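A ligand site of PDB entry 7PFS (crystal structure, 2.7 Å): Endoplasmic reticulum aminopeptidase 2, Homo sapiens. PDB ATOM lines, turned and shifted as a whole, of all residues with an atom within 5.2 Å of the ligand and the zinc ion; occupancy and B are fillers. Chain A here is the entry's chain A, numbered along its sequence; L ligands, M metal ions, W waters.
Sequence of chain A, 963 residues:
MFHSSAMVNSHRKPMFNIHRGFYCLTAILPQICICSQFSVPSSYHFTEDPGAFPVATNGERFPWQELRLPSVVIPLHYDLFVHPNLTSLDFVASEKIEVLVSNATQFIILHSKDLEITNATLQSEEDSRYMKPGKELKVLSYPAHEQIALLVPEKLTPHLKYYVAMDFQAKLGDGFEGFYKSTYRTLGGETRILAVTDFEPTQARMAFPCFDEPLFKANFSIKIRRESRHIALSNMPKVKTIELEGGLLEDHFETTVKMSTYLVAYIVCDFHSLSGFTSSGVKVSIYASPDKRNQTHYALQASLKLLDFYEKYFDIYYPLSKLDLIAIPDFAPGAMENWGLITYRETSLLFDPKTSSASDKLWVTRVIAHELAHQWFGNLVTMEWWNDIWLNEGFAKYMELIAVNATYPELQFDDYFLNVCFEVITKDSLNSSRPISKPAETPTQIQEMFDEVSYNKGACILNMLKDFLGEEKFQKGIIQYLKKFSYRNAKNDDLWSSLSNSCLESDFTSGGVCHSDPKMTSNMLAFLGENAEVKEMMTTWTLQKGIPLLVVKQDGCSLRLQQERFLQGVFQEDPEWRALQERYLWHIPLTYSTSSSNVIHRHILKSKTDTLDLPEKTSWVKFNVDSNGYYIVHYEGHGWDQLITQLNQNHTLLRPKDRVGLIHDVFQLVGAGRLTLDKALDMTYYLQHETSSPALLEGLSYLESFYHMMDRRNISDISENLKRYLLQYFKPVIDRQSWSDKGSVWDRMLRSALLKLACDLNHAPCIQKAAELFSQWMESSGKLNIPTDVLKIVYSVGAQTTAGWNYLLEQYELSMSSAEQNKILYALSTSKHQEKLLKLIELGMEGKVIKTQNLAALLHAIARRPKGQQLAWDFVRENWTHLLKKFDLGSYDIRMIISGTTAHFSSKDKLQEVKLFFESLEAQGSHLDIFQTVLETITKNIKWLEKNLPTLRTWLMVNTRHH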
ATOM      1  N   ASP A 198      31.876  12.154   3.706  1.00  0.00           N
ATOM      2  CA  ASP A 198      31.138  11.836   4.932  1.00  0.00           C
ATOM      3  C   ASP A 198      29.642  11.779   4.625  1.00  0.00           C
ATOM      4  O   ASP A 198      29.042  12.782   4.258  1.00  0.00           O
ATOM      5  CB  ASP A 198      31.388  12.862   6.040  1.00  0.00           C
ATOM      6  CG  ASP A 198      31.012  12.337   7.405  1.00  0.00           C
ATOM      7  OD1 ASP A 198      31.820  11.510   7.922  1.00  0.00           O
ATOM      8  OD2 ASP A 198      29.902  12.720   7.909  1.00  0.00           O
ATOM      9  N   GLU A 200      26.857   9.736   6.559  1.00  0.00           N
ATOM     10  CA  GLU A 200      25.766   9.548   7.509  1.00  0.00           C
ATOM     11  C   GLU A 200      25.210  10.881   7.983  1.00  0.00           C
ATOM     12  O   GLU A 200      25.971  11.816   8.301  1.00  0.00           O
ATOM     13  CB  GLU A 200      26.188   8.739   8.729  1.00  0.00           C
ATOM     14  CG  GLU A 200      25.035   7.987   9.333  1.00  0.00           C
ATOM     15  CD  GLU A 200      25.457   7.115  10.501  1.00  0.00           C
ATOM     16  OE1 GLU A 200      26.660   7.160  10.875  1.00  0.00           O
ATOM     17  OE2 GLU A 200      24.572   6.394  11.062  1.00  0.00           O
ATOM     18  N   PRO A 201      23.878  11.027   8.029  1.00  0.00           N
ATOM     19  CA  PRO A 201      22.980   9.914   7.634  1.00  0.00           C
ATOM     20  C   PRO A 201      22.478   9.883   6.187  1.00  0.00           C
ATOM     21  O   PRO A 201      22.289   8.763   5.700  1.00  0.00           O
ATOM     22  CB  PRO A 201      21.784  10.072   8.574  1.00  0.00           C
ATOM     23  CG  PRO A 201      21.776  11.532   8.916  1.00  0.00           C
ATOM     24  CD  PRO A 201      23.186  12.076   8.798  1.00  0.00           C
ATOM     25  N   ALA A 332      33.867  17.467  10.749  1.00  0.00           N
ATOM     26  CA  ALA A 332      32.706  17.882  11.554  1.00  0.00           C
ATOM     27  C   ALA A 332      32.291  16.854  12.595  1.00  0.00           C
ATOM     28  O   ALA A 332      32.129  17.214  13.778  1.00  0.00           O
ATOM     29  CB  ALA A 332      31.538  18.199  10.636  1.00  0.00           C
ATOM     30  N   PRO A 333      32.068  15.585  12.241  1.00  0.00           N
ATOM     31  CA  PRO A 333      31.513  14.654  13.231  1.00  0.00           C
ATOM     32  C   PRO A 333      32.453  14.263  14.394  1.00  0.00           C
ATOM     33  O   PRO A 333      31.979  13.970  15.490  1.00  0.00           O
ATOM     34  CB  PRO A 333      31.176  13.403  12.394  1.00  0.00           C
ATOM     35  CG  PRO A 333      31.205  13.872  10.948  1.00  0.00           C
ATOM     36  CD  PRO A 333      32.226  14.976  10.917  1.00  0.00           C
ATOM     37  N   GLY A 334      33.745  14.323  14.296  1.00  0.00           N
ATOM     38  CA  GLY A 334      34.349  13.596  15.423  1.00  0.00           C
ATOM     39  C   GLY A 334      34.801  12.150  15.193  1.00  0.00           C
ATOM     40  O   GLY A 334      35.970  11.838  15.437  1.00  0.00           O
ATOM     41  N   ALA A 335      33.933  11.287  14.665  1.00  0.00           N
ATOM     42  CA  ALA A 335      34.334  10.004  14.129  1.00  0.00           C
ATOM     43  C   ALA A 335      33.220   9.466  13.223  1.00  0.00           C
ATOM     44  O   ALA A 335      32.045   9.814  13.412  1.00  0.00           O
ATOM     45  CB  ALA A 335      34.642   9.012  15.242  1.00  0.00           C
ATOM     46  N   MET A 336      33.583   8.625  12.252  1.00  0.00           N
ATOM     47  CA  MET A 336      32.613   8.099  11.304  1.00  0.00           C
ATOM     48  C   MET A 336      33.110   6.731  10.891  1.00  0.00           C
ATOM     49  O   MET A 336      34.178   6.641  10.280  1.00  0.00           O
ATOM     50  CB  MET A 336      32.460   8.972  10.059  1.00  0.00           C
ATOM     51  CG  MET A 336      31.413   8.437   9.065  1.00  0.00           C
ATOM     52  SD  MET A 336      29.885   7.781   9.858  1.00  0.00           S
ATOM     53  CE  MET A 336      29.493   6.444   8.739  1.00  0.00           C
ATOM     54  N   GLU A 337      32.250   5.705  11.073  1.00  0.00           N
ATOM     55  CA  GLU A 337      32.682   4.306  11.175  1.00  0.00           C
ATOM     56  C   GLU A 337      32.683   3.612   9.824  1.00  0.00           C
ATOM     57  O   GLU A 337      32.376   2.415   9.765  1.00  0.00           O
ATOM     58  CB  GLU A 337      31.785   3.543  12.168  1.00  0.00           C
ATOM     59  CG  GLU A 337      30.346   3.165  11.607  1.00  0.00           C
ATOM     60  CD  GLU A 337      29.195   4.125  11.990  1.00  0.00           C
ATOM     61  OE1 GLU A 337      29.472   5.218  12.557  1.00  0.00           O
ATOM     62  OE2 GLU A 337      28.011   3.775  11.713  1.00  0.00           O
ATOM     63  N   ARG A 345      38.244  12.989  13.857  1.00  0.00           N
ATOM     64  CA  ARG A 345      38.907  14.202  14.312  1.00  0.00           C
ATOM     65  C   ARG A 345      40.275  13.844  14.878  1.00  0.00           C
ATOM     66  O   ARG A 345      40.431  12.848  15.609  1.00  0.00           O
ATOM     67  CB  ARG A 345      38.067  14.864  15.399  1.00  0.00           C
ATOM     68  CG  ARG A 345      37.085  15.854  14.885  1.00  0.00           C
ATOM     69  CD  ARG A 345      36.500  16.591  16.012  1.00  0.00           C
ATOM     70  NE  ARG A 345      35.384  17.383  15.542  1.00  0.00           N
ATOM     71  CZ  ARG A 345      34.891  18.418  16.221  1.00  0.00           C
ATOM     72  NH1 ARG A 345      35.451  18.760  17.376  1.00  0.00           N
ATOM     73  NH2 ARG A 345      33.837  19.081  15.764  1.00  0.00           N
ATOM     74  N   TRP A 363      39.927   9.573  26.253  1.00  0.00           N
ATOM     75  CA  TRP A 363      38.983   9.932  25.201  1.00  0.00           C
ATOM     76  C   TRP A 363      39.314   9.204  23.911  1.00  0.00           C
ATOM     77  O   TRP A 363      38.441   8.598  23.265  1.00  0.00           O
ATOM     78  CB  TRP A 363      38.984  11.445  25.001  1.00  0.00           C
ATOM     79  CG  TRP A 363      38.197  11.973  23.816  1.00  0.00           C
ATOM     80  CD1 TRP A 363      38.704  12.604  22.706  1.00  0.00           C
ATOM     81  CD2 TRP A 363      36.773  11.914  23.619  1.00  0.00           C
ATOM     82  NE1 TRP A 363      37.690  12.937  21.841  1.00  0.00           N
ATOM     83  CE2 TRP A 363      36.499  12.517  22.369  1.00  0.00           C
ATOM     84  CE3 TRP A 363      35.706  11.413  24.366  1.00  0.00           C
ATOM     85  CZ2 TRP A 363      35.205  12.644  21.860  1.00  0.00           C
ATOM     86  CZ3 TRP A 363      34.430  11.553  23.860  1.00  0.00           C
ATOM     87  CH2 TRP A 363      34.191  12.158  22.621  1.00  0.00           C
ATOM     88  N   HIS A 370      34.726   2.798  20.258  1.00  0.00           N
ATOM     89  CA  HIS A 370      33.393   3.047  19.730  1.00  0.00           C
ATOM     90  C   HIS A 370      33.334   2.755  18.232  1.00  0.00           C
ATOM     91  O   HIS A 370      32.524   1.937  17.798  1.00  0.00           O
ATOM     92  CB  HIS A 370      32.999   4.480  20.014  1.00  0.00           C
ATOM     93  CG  HIS A 370      31.607   4.828  19.603  1.00  0.00           C
ATOM     94  ND1 HIS A 370      30.554   4.813  20.486  1.00  0.00           N
ATOM     95  CD2 HIS A 370      31.101   5.227  18.419  1.00  0.00           C
ATOM     96  CE1 HIS A 370      29.456   5.177  19.856  1.00  0.00           C
ATOM     97  NE2 HIS A 370      29.761   5.437  18.601  1.00  0.00           N
ATOM     98  N   GLU A 371      34.188   3.388  17.434  1.00  0.00           N
ATOM     99  CA  GLU A 371      34.164   3.144  15.985  1.00  0.00           C
ATOM    100  C   GLU A 371      34.315   1.664  15.657  1.00  0.00           C
ATOM    101  O   GLU A 371      33.643   1.170  14.732  1.00  0.00           O
ATOM    102  CB  GLU A 371      35.251   3.941  15.262  1.00  0.00           C
ATOM    103  CG  GLU A 371      34.990   5.454  15.184  1.00  0.00           C
ATOM    104  CD  GLU A 371      33.507   5.876  15.356  1.00  0.00           C
ATOM    105  OE1 GLU A 371      33.218   6.483  16.409  1.00  0.00           O
ATOM    106  OE2 GLU A 371      32.667   5.643  14.449  1.00  0.00           O
ATOM    107  N   HIS A 374      31.239  -0.397  15.847  1.00  0.00           N
ATOM    108  CA  HIS A 374      30.325  -0.168  14.743  1.00  0.00           C
ATOM    109  C   HIS A 374      30.564  -1.125  13.573  1.00  0.00           C
ATOM    110  O   HIS A 374      29.647  -1.348  12.765  1.00  0.00           O
ATOM    111  CB  HIS A 374      30.465   1.250  14.238  1.00  0.00           C
ATOM    112  CG  HIS A 374      29.604   2.214  14.950  1.00  0.00           C
ATOM    113  ND1 HIS A 374      28.275   1.949  15.209  1.00  0.00           N
ATOM    114  CD2 HIS A 374      29.858   3.439  15.462  1.00  0.00           C
ATOM    115  CE1 HIS A 374      27.763   2.977  15.862  1.00  0.00           C
ATOM    116  NE2 HIS A 374      28.709   3.891  16.049  1.00  0.00           N
ATOM    117  N   GLU A 393      23.912   2.946  17.609  1.00  0.00           N
ATOM    118  CA  GLU A 393      24.671   3.806  18.500  1.00  0.00           C
ATOM    119  C   GLU A 393      24.545   3.360  19.934  1.00  0.00           C
ATOM    120  O   GLU A 393      25.500   3.479  20.703  1.00  0.00           O
ATOM    121  CB  GLU A 393      24.258   5.267  18.321  1.00  0.00           C
ATOM    122  CG  GLU A 393      24.775   5.888  17.010  1.00  0.00           C
ATOM    123  CD  GLU A 393      26.275   5.746  16.786  1.00  0.00           C
ATOM    124  OE1 GLU A 393      26.677   6.096  15.681  1.00  0.00           O
ATOM    125  OE2 GLU A 393      27.069   5.314  17.656  1.00  0.00           O
ATOM    126  N   ALA A 396      27.190   0.292  20.081  1.00  0.00           N
ATOM    127  CA  ALA A 396      28.555   0.803  20.053  1.00  0.00           C
ATOM    128  C   ALA A 396      28.855   1.544  21.339  1.00  0.00           C
ATOM    129  O   ALA A 396      29.904   1.332  21.938  1.00  0.00           O
ATOM    130  CB  ALA A 396      28.793   1.706  18.850  1.00  0.00           C
ATOM    131  N   GLN A 447      18.468  13.233  11.681  1.00  0.00           N
ATOM    132  CA  GLN A 447      19.661  13.532  12.475  1.00  0.00           C
ATOM    133  C   GLN A 447      19.313  13.841  13.914  1.00  0.00           C
ATOM    134  O   GLN A 447      20.092  13.514  14.806  1.00  0.00           O
ATOM    135  CB  GLN A 447      20.502  14.658  11.871  1.00  0.00           C
ATOM    136  CG  GLN A 447      19.807  15.651  10.961  1.00  0.00           C
ATOM    137  CD  GLN A 447      20.801  16.526  10.200  1.00  0.00           C
ATOM    138  OE1 GLN A 447      22.034  16.306  10.301  1.00  0.00           O
ATOM    139  NE2 GLN A 447      20.292  17.542   9.460  1.00  0.00           N
ATOM    140  N   PHE A 450      20.024  11.226  16.566  1.00  0.00           N
ATOM    141  CA  PHE A 450      21.318  10.951  17.182  1.00  0.00           C
ATOM    142  C   PHE A 450      21.449  11.884  18.384  1.00  0.00           C
ATOM    143  O   PHE A 450      21.942  13.003  18.272  1.00  0.00           O
ATOM    144  CB  PHE A 450      22.463  11.177  16.200  1.00  0.00           C
ATOM    145  CG  PHE A 450      22.504  10.189  15.084  1.00  0.00           C
ATOM    146  CD1 PHE A 450      21.691  10.352  13.991  1.00  0.00           C
ATOM    147  CD2 PHE A 450      23.356   9.123  15.120  1.00  0.00           C
ATOM    148  CE1 PHE A 450      21.748   9.470  12.963  1.00  0.00           C
ATOM    149  CE2 PHE A 450      23.429   8.222  14.076  1.00  0.00           C
ATOM    150  CZ  PHE A 450      22.627   8.398  12.977  1.00  0.00           C
ATOM    151  N   ASP A 451      21.023  11.402  19.555  1.00  0.00           N
ATOM    152  CA  ASP A 451      21.043  12.244  20.744  1.00  0.00           C
ATOM    153  C   ASP A 451      21.481  11.415  21.949  1.00  0.00           C
ATOM    154  O   ASP A 451      21.922  10.260  21.830  1.00  0.00           O
ATOM    155  CB  ASP A 451      19.663  12.888  20.963  1.00  0.00           C
ATOM    156  CG  ASP A 451      18.547  11.869  21.264  1.00  0.00           C
ATOM    157  OD1 ASP A 451      18.814  10.711  21.671  1.00  0.00           O
ATOM    158  OD2 ASP A 451      17.364  12.277  21.091  1.00  0.00           O
ATOM    159  N   GLU A 452      21.311  12.004  23.137  1.00  0.00           N
ATOM    160  CA  GLU A 452      21.614  11.307  24.383  1.00  0.00           C
ATOM    161  C   GLU A 452      20.750  10.060  24.557  1.00  0.00           C
ATOM    162  O   GLU A 452      21.162   9.104  25.243  1.00  0.00           O
ATOM    163  CB  GLU A 452      21.410  12.244  25.573  1.00  0.00           C
ATOM    164  CG  GLU A 452      22.653  12.936  26.059  1.00  0.00           C
ATOM    165  CD  GLU A 452      22.897  14.270  25.368  1.00  0.00           C
ATOM    166  OE1 GLU A 452      22.120  14.647  24.435  1.00  0.00           O
ATOM    167  OE2 GLU A 452      23.881  14.947  25.754  1.00  0.00           O
ATOM    168  N   TYR A 455      22.067   7.097  22.204  1.00  0.00           N
ATOM    169  CA  TYR A 455      23.380   6.610  22.618  1.00  0.00           C
ATOM    170  C   TYR A 455      23.371   6.167  24.067  1.00  0.00           C
ATOM    171  O   TYR A 455      23.582   4.987  24.372  1.00  0.00           O
ATOM    172  CB  TYR A 455      24.412   7.722  22.530  1.00  0.00           C
ATOM    173  CG  TYR A 455      24.907   8.036  21.167  1.00  0.00           C
ATOM    174  CD1 TYR A 455      24.113   8.738  20.281  1.00  0.00           C
ATOM    175  CD2 TYR A 455      26.189   7.651  20.775  1.00  0.00           C
ATOM    176  CE1 TYR A 455      24.583   9.050  19.027  1.00  0.00           C
ATOM    177  CE2 TYR A 455      26.647   7.954  19.540  1.00  0.00           C
ATOM    178  CZ  TYR A 455      25.842   8.654  18.662  1.00  0.00           C
ATOM    179  OH  TYR A 455      26.300   8.953  17.414  1.00  0.00           O
ATOM    180  N   ASN A 456      23.099   7.116  24.954  1.00  0.00           N
ATOM    181  CA  ASN A 456      23.390   6.938  26.363  1.00  0.00           C
ATOM    182  C   ASN A 456      22.351   6.037  27.001  1.00  0.00           C
ATOM    183  O   ASN A 456      22.700   4.984  27.560  1.00  0.00           O
ATOM    184  CB  ASN A 456      23.446   8.299  27.055  1.00  0.00           C
ATOM    185  CG  ASN A 456      24.671   9.090  26.660  1.00  0.00           C
ATOM    186  OD1 ASN A 456      25.107   9.096  25.491  1.00  0.00           O
ATOM    187  ND2 ASN A 456      25.236   9.778  27.633  1.00  0.00           N
ATOM    188  N   TYR A 892      24.463  18.868  14.608  1.00  0.00           N
ATOM    189  CA  TYR A 892      24.942  18.942  15.981  1.00  0.00           C
ATOM    190  C   TYR A 892      25.524  20.306  16.301  1.00  0.00           C
ATOM    191  O   TYR A 892      25.381  20.813  17.413  1.00  0.00           O
ATOM    192  CB  TYR A 892      26.003  17.869  16.227  1.00  0.00           C
ATOM    193  CG  TYR A 892      26.351  17.659  17.674  1.00  0.00           C
ATOM    194  CD1 TYR A 892      25.387  17.229  18.601  1.00  0.00           C
ATOM    195  CD2 TYR A 892      27.657  17.904  18.142  1.00  0.00           C
ATOM    196  CE1 TYR A 892      25.721  17.039  19.936  1.00  0.00           C
ATOM    197  CE2 TYR A 892      28.007  17.705  19.487  1.00  0.00           C
ATOM    198  CZ  TYR A 892      27.025  17.265  20.388  1.00  0.00           C
ATOM    199  OH  TYR A 892      27.346  17.070  21.718  1.00  0.00           O
ATOM    200  N   ARG A 895      22.762  22.462  17.225  1.00  0.00           N
ATOM    201  CA  ARG A 895      22.180  22.027  18.486  1.00  0.00           C
ATOM    202  C   ARG A 895      22.979  22.554  19.679  1.00  0.00           C
ATOM    203  O   ARG A 895      22.400  23.011  20.677  1.00  0.00           O
ATOM    204  CB  ARG A 895      22.117  20.502  18.566  1.00  0.00           C
ATOM    205  CG  ARG A 895      21.340  19.961  19.771  1.00  0.00           C
ATOM    206  CD  ARG A 895      21.352  18.433  19.832  1.00  0.00           C
ATOM    207  NE  ARG A 895      20.790  17.835  18.622  1.00  0.00           N
ATOM    208  CZ  ARG A 895      21.089  16.614  18.189  1.00  0.00           C
ATOM    209  NH1 ARG A 895      21.930  15.857  18.874  1.00  0.00           N
ATOM    210  NH2 ARG A 895      20.534  16.158  17.069  1.00  0.00           N
HETATM  211  C1  LIG L   1      27.203  12.969  15.227  1.00  0.00           C
HETATM  212  C2  LIG L   1      26.241  12.967  17.762  1.00  0.00           C
HETATM  213  C3  LIG L   1      29.358  11.444  19.944  1.00  0.00           C
HETATM  214  C4  LIG L   1      28.924  12.592  20.615  1.00  0.00           C
HETATM  215  C5  LIG L   1      27.533  12.593  21.248  1.00  0.00           C
HETATM  216  C6  LIG L   1      25.501  13.835  21.736  1.00  0.00           C
HETATM  217  C7  LIG L   1      25.697  11.499  22.343  1.00  0.00           C
HETATM  218  C8  LIG L   1      29.741  13.719  20.655  1.00  0.00           C
HETATM  219  C9  LIG L   1      28.962   8.184  14.122  1.00  0.00           C
HETATM  220  C10 LIG L   1      30.795   8.988  16.390  1.00  0.00           C
HETATM  221  C11 LIG L   1      30.240   9.959  17.445  1.00  0.00           C
HETATM  222  C12 LIG L   1      30.073  11.218  16.730  1.00  0.00           C
HETATM  223  C13 LIG L   1      28.659  12.996  15.774  1.00  0.00           C
HETATM  224  C14 LIG L   1      26.204  13.339  16.281  1.00  0.00           C
HETATM  225  C15 LIG L   1      25.812  14.746  15.985  1.00  0.00           C
HETATM  226  C16 LIG L   1      28.903  14.303  16.325  1.00  0.00           C
HETATM  227  C17 LIG L   1      31.093  10.160  18.627  1.00  0.00           C
HETATM  228  C18 LIG L   1      30.638  11.415  19.351  1.00  0.00           C
HETATM  229  C19 LIG L   1      26.793  13.776  21.191  1.00  0.00           C
HETATM  230  C20 LIG L   1      24.959  12.693  22.313  1.00  0.00           C
HETATM  231  C21 LIG L   1      26.985  11.452  21.817  1.00  0.00           C
HETATM  232  C22 LIG L   1      31.001  13.659  20.044  1.00  0.00           C
HETATM  233  C23 LIG L   1      31.953  14.835  20.043  1.00  0.00           C
HETATM  234  C24 LIG L   1      31.976  15.600  18.896  1.00  0.00           C
HETATM  235  C25 LIG L   1      32.816  16.693  18.834  1.00  0.00           C
HETATM  236  C26 LIG L   1      33.643  16.971  19.951  1.00  0.00           C
HETATM  237  C27 LIG L   1      33.613  16.190  21.112  1.00  0.00           C
HETATM  238  C28 LIG L   1      32.762  15.096  21.183  1.00  0.00           C
HETATM  239  C29 LIG L   1      31.454  12.529  19.388  1.00  0.00           C
HETATM  240  C30 LIG L   1      28.330   9.533  14.020  1.00  0.00           C
HETATM  241  C31 LIG L   1      28.145  10.013  12.561  1.00  0.00           C
HETATM  242  C32 LIG L   1      27.105  11.123  12.345  1.00  0.00           C
HETATM  243  C33 LIG L   1      27.502  12.399  12.022  1.00  0.00           C
HETATM  244  C34 LIG L   1      26.522  13.406  11.879  1.00  0.00           C
HETATM  245  C35 LIG L   1      25.155  13.110  12.084  1.00  0.00           C
HETATM  246  C36 LIG L   1      24.767  11.812  12.407  1.00  0.00           C
HETATM  247  C37 LIG L   1      25.742  10.806  12.543  1.00  0.00           C
HETATM  248  N1  LIG L   1      27.932   7.223  13.950  1.00  0.00           N
HETATM  249  N2  LIG L   1      28.762  11.788  16.549  1.00  0.00           N
HETATM  250  N3  LIG L   1      28.862  15.381  15.398  1.00  0.00           N
HETATM  251  O1  LIG L   1      30.173   6.318  15.734  1.00  0.00           O
HETATM  252  O2  LIG L   1      28.979  14.493  17.519  1.00  0.00           O
HETATM  253  O3  LIG L   1      31.072  11.771  16.262  1.00  0.00           O
HETATM  254  O4  LIG L   1      28.447   7.657  16.674  1.00  0.00           O
HETATM  255  P1  LIG L   1      29.584   7.732  15.742  1.00  0.00           P
HETATM  256 ZN    ZN M   1      28.595   5.732  16.950  1.00  0.00          ZN
HETATM  257  O   HOH W   1      25.837   4.874  13.079  1.00  0.00           O
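N3 of the ligand lies close to O of Pro 333 (3.4 Å). The side-chain hydroxyl (OH) of Tyr 455 sits close to an oxygen (O4) of the ligand. The side-chain carboxylate of Glu 337 lies within salt-bridge range of a nitrogen (N1) of the ligand. The backbone NH (N) of Ala 335 is in hydrogen-bond range of an oxygen (O3) of the ligand, at 3.3 Å. OE1 of Glu 200 lies within salt-bridge range of N1 of the ligand, 3.3 Å away.
The side-chain hydroxyl of Tyr 455 lies close to the side-chain carboxylate of Glu 393 (3.4 Å). The side-chain carboxylate (OE2) of Glu 371 sits close to the backbone NH (N) of Glu 337 (3.4 Å). O of Gly 334 is in hydrogen-bond range of N of Arg 345. The guanidinium group of Arg 345 is in hydrogen-bond range of the backbone carbonyl oxygen of Ala 332 (3.2 Å). O of Phe 450 is in hydrogen-bond range of NH1 of Arg 895 (2.9 Å).
Water W1 lies within hydrogen-bond range of OE2 of Glu 337 (2.8 Å), OE2 of Glu 200 (2.8 Å) and N1 of the ligand (3.3 Å).
OE2 of Glu 371 lies close to O1 of the ligand (2.9 Å). Merely in contact with the ligand: Tyr 892 (3.1 Å), Trp 363 (3.5 Å), Arg 345 (3.6 Å), Asp 451 (3.7 Å), Phe 450 (3.8 Å), Glu 452 (3.8 Å), Gly 334 (3.8 Å), Met 336 (3.9 Å) and Pro 201 (3.9 Å). Hydrophobic or aromatic side chains that line the ligand: Pro 201, Pro 333, Met 336, Trp 363, His 370, His 374, Phe 450, Tyr 455 and Tyr 892. Of the 24 residues printed, 18 come within 4 Å of the ligand.
Merely in contact with the zinc ion: Tyr 455. Within 4 Å of the zinc ion: His 370, His 374, Glu 393 and Tyr 455.
The zinc ion is bound by OE2 of Glu 393, at 1.7 Å. The zinc ion is bound by O4 of the ligand, 2.0 Å away. The zinc ion is bound by NE2 of His 370, at 2.0 Å. NE2 of His 374 is bound to the zinc ion (2.1 Å). O1 of the ligand is bound to the zinc ion (2.1 Å). OE1 of Glu 393 is bound to the zinc ion, 2.3 Å away. The zinc ion has six donor atoms within binding distance.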
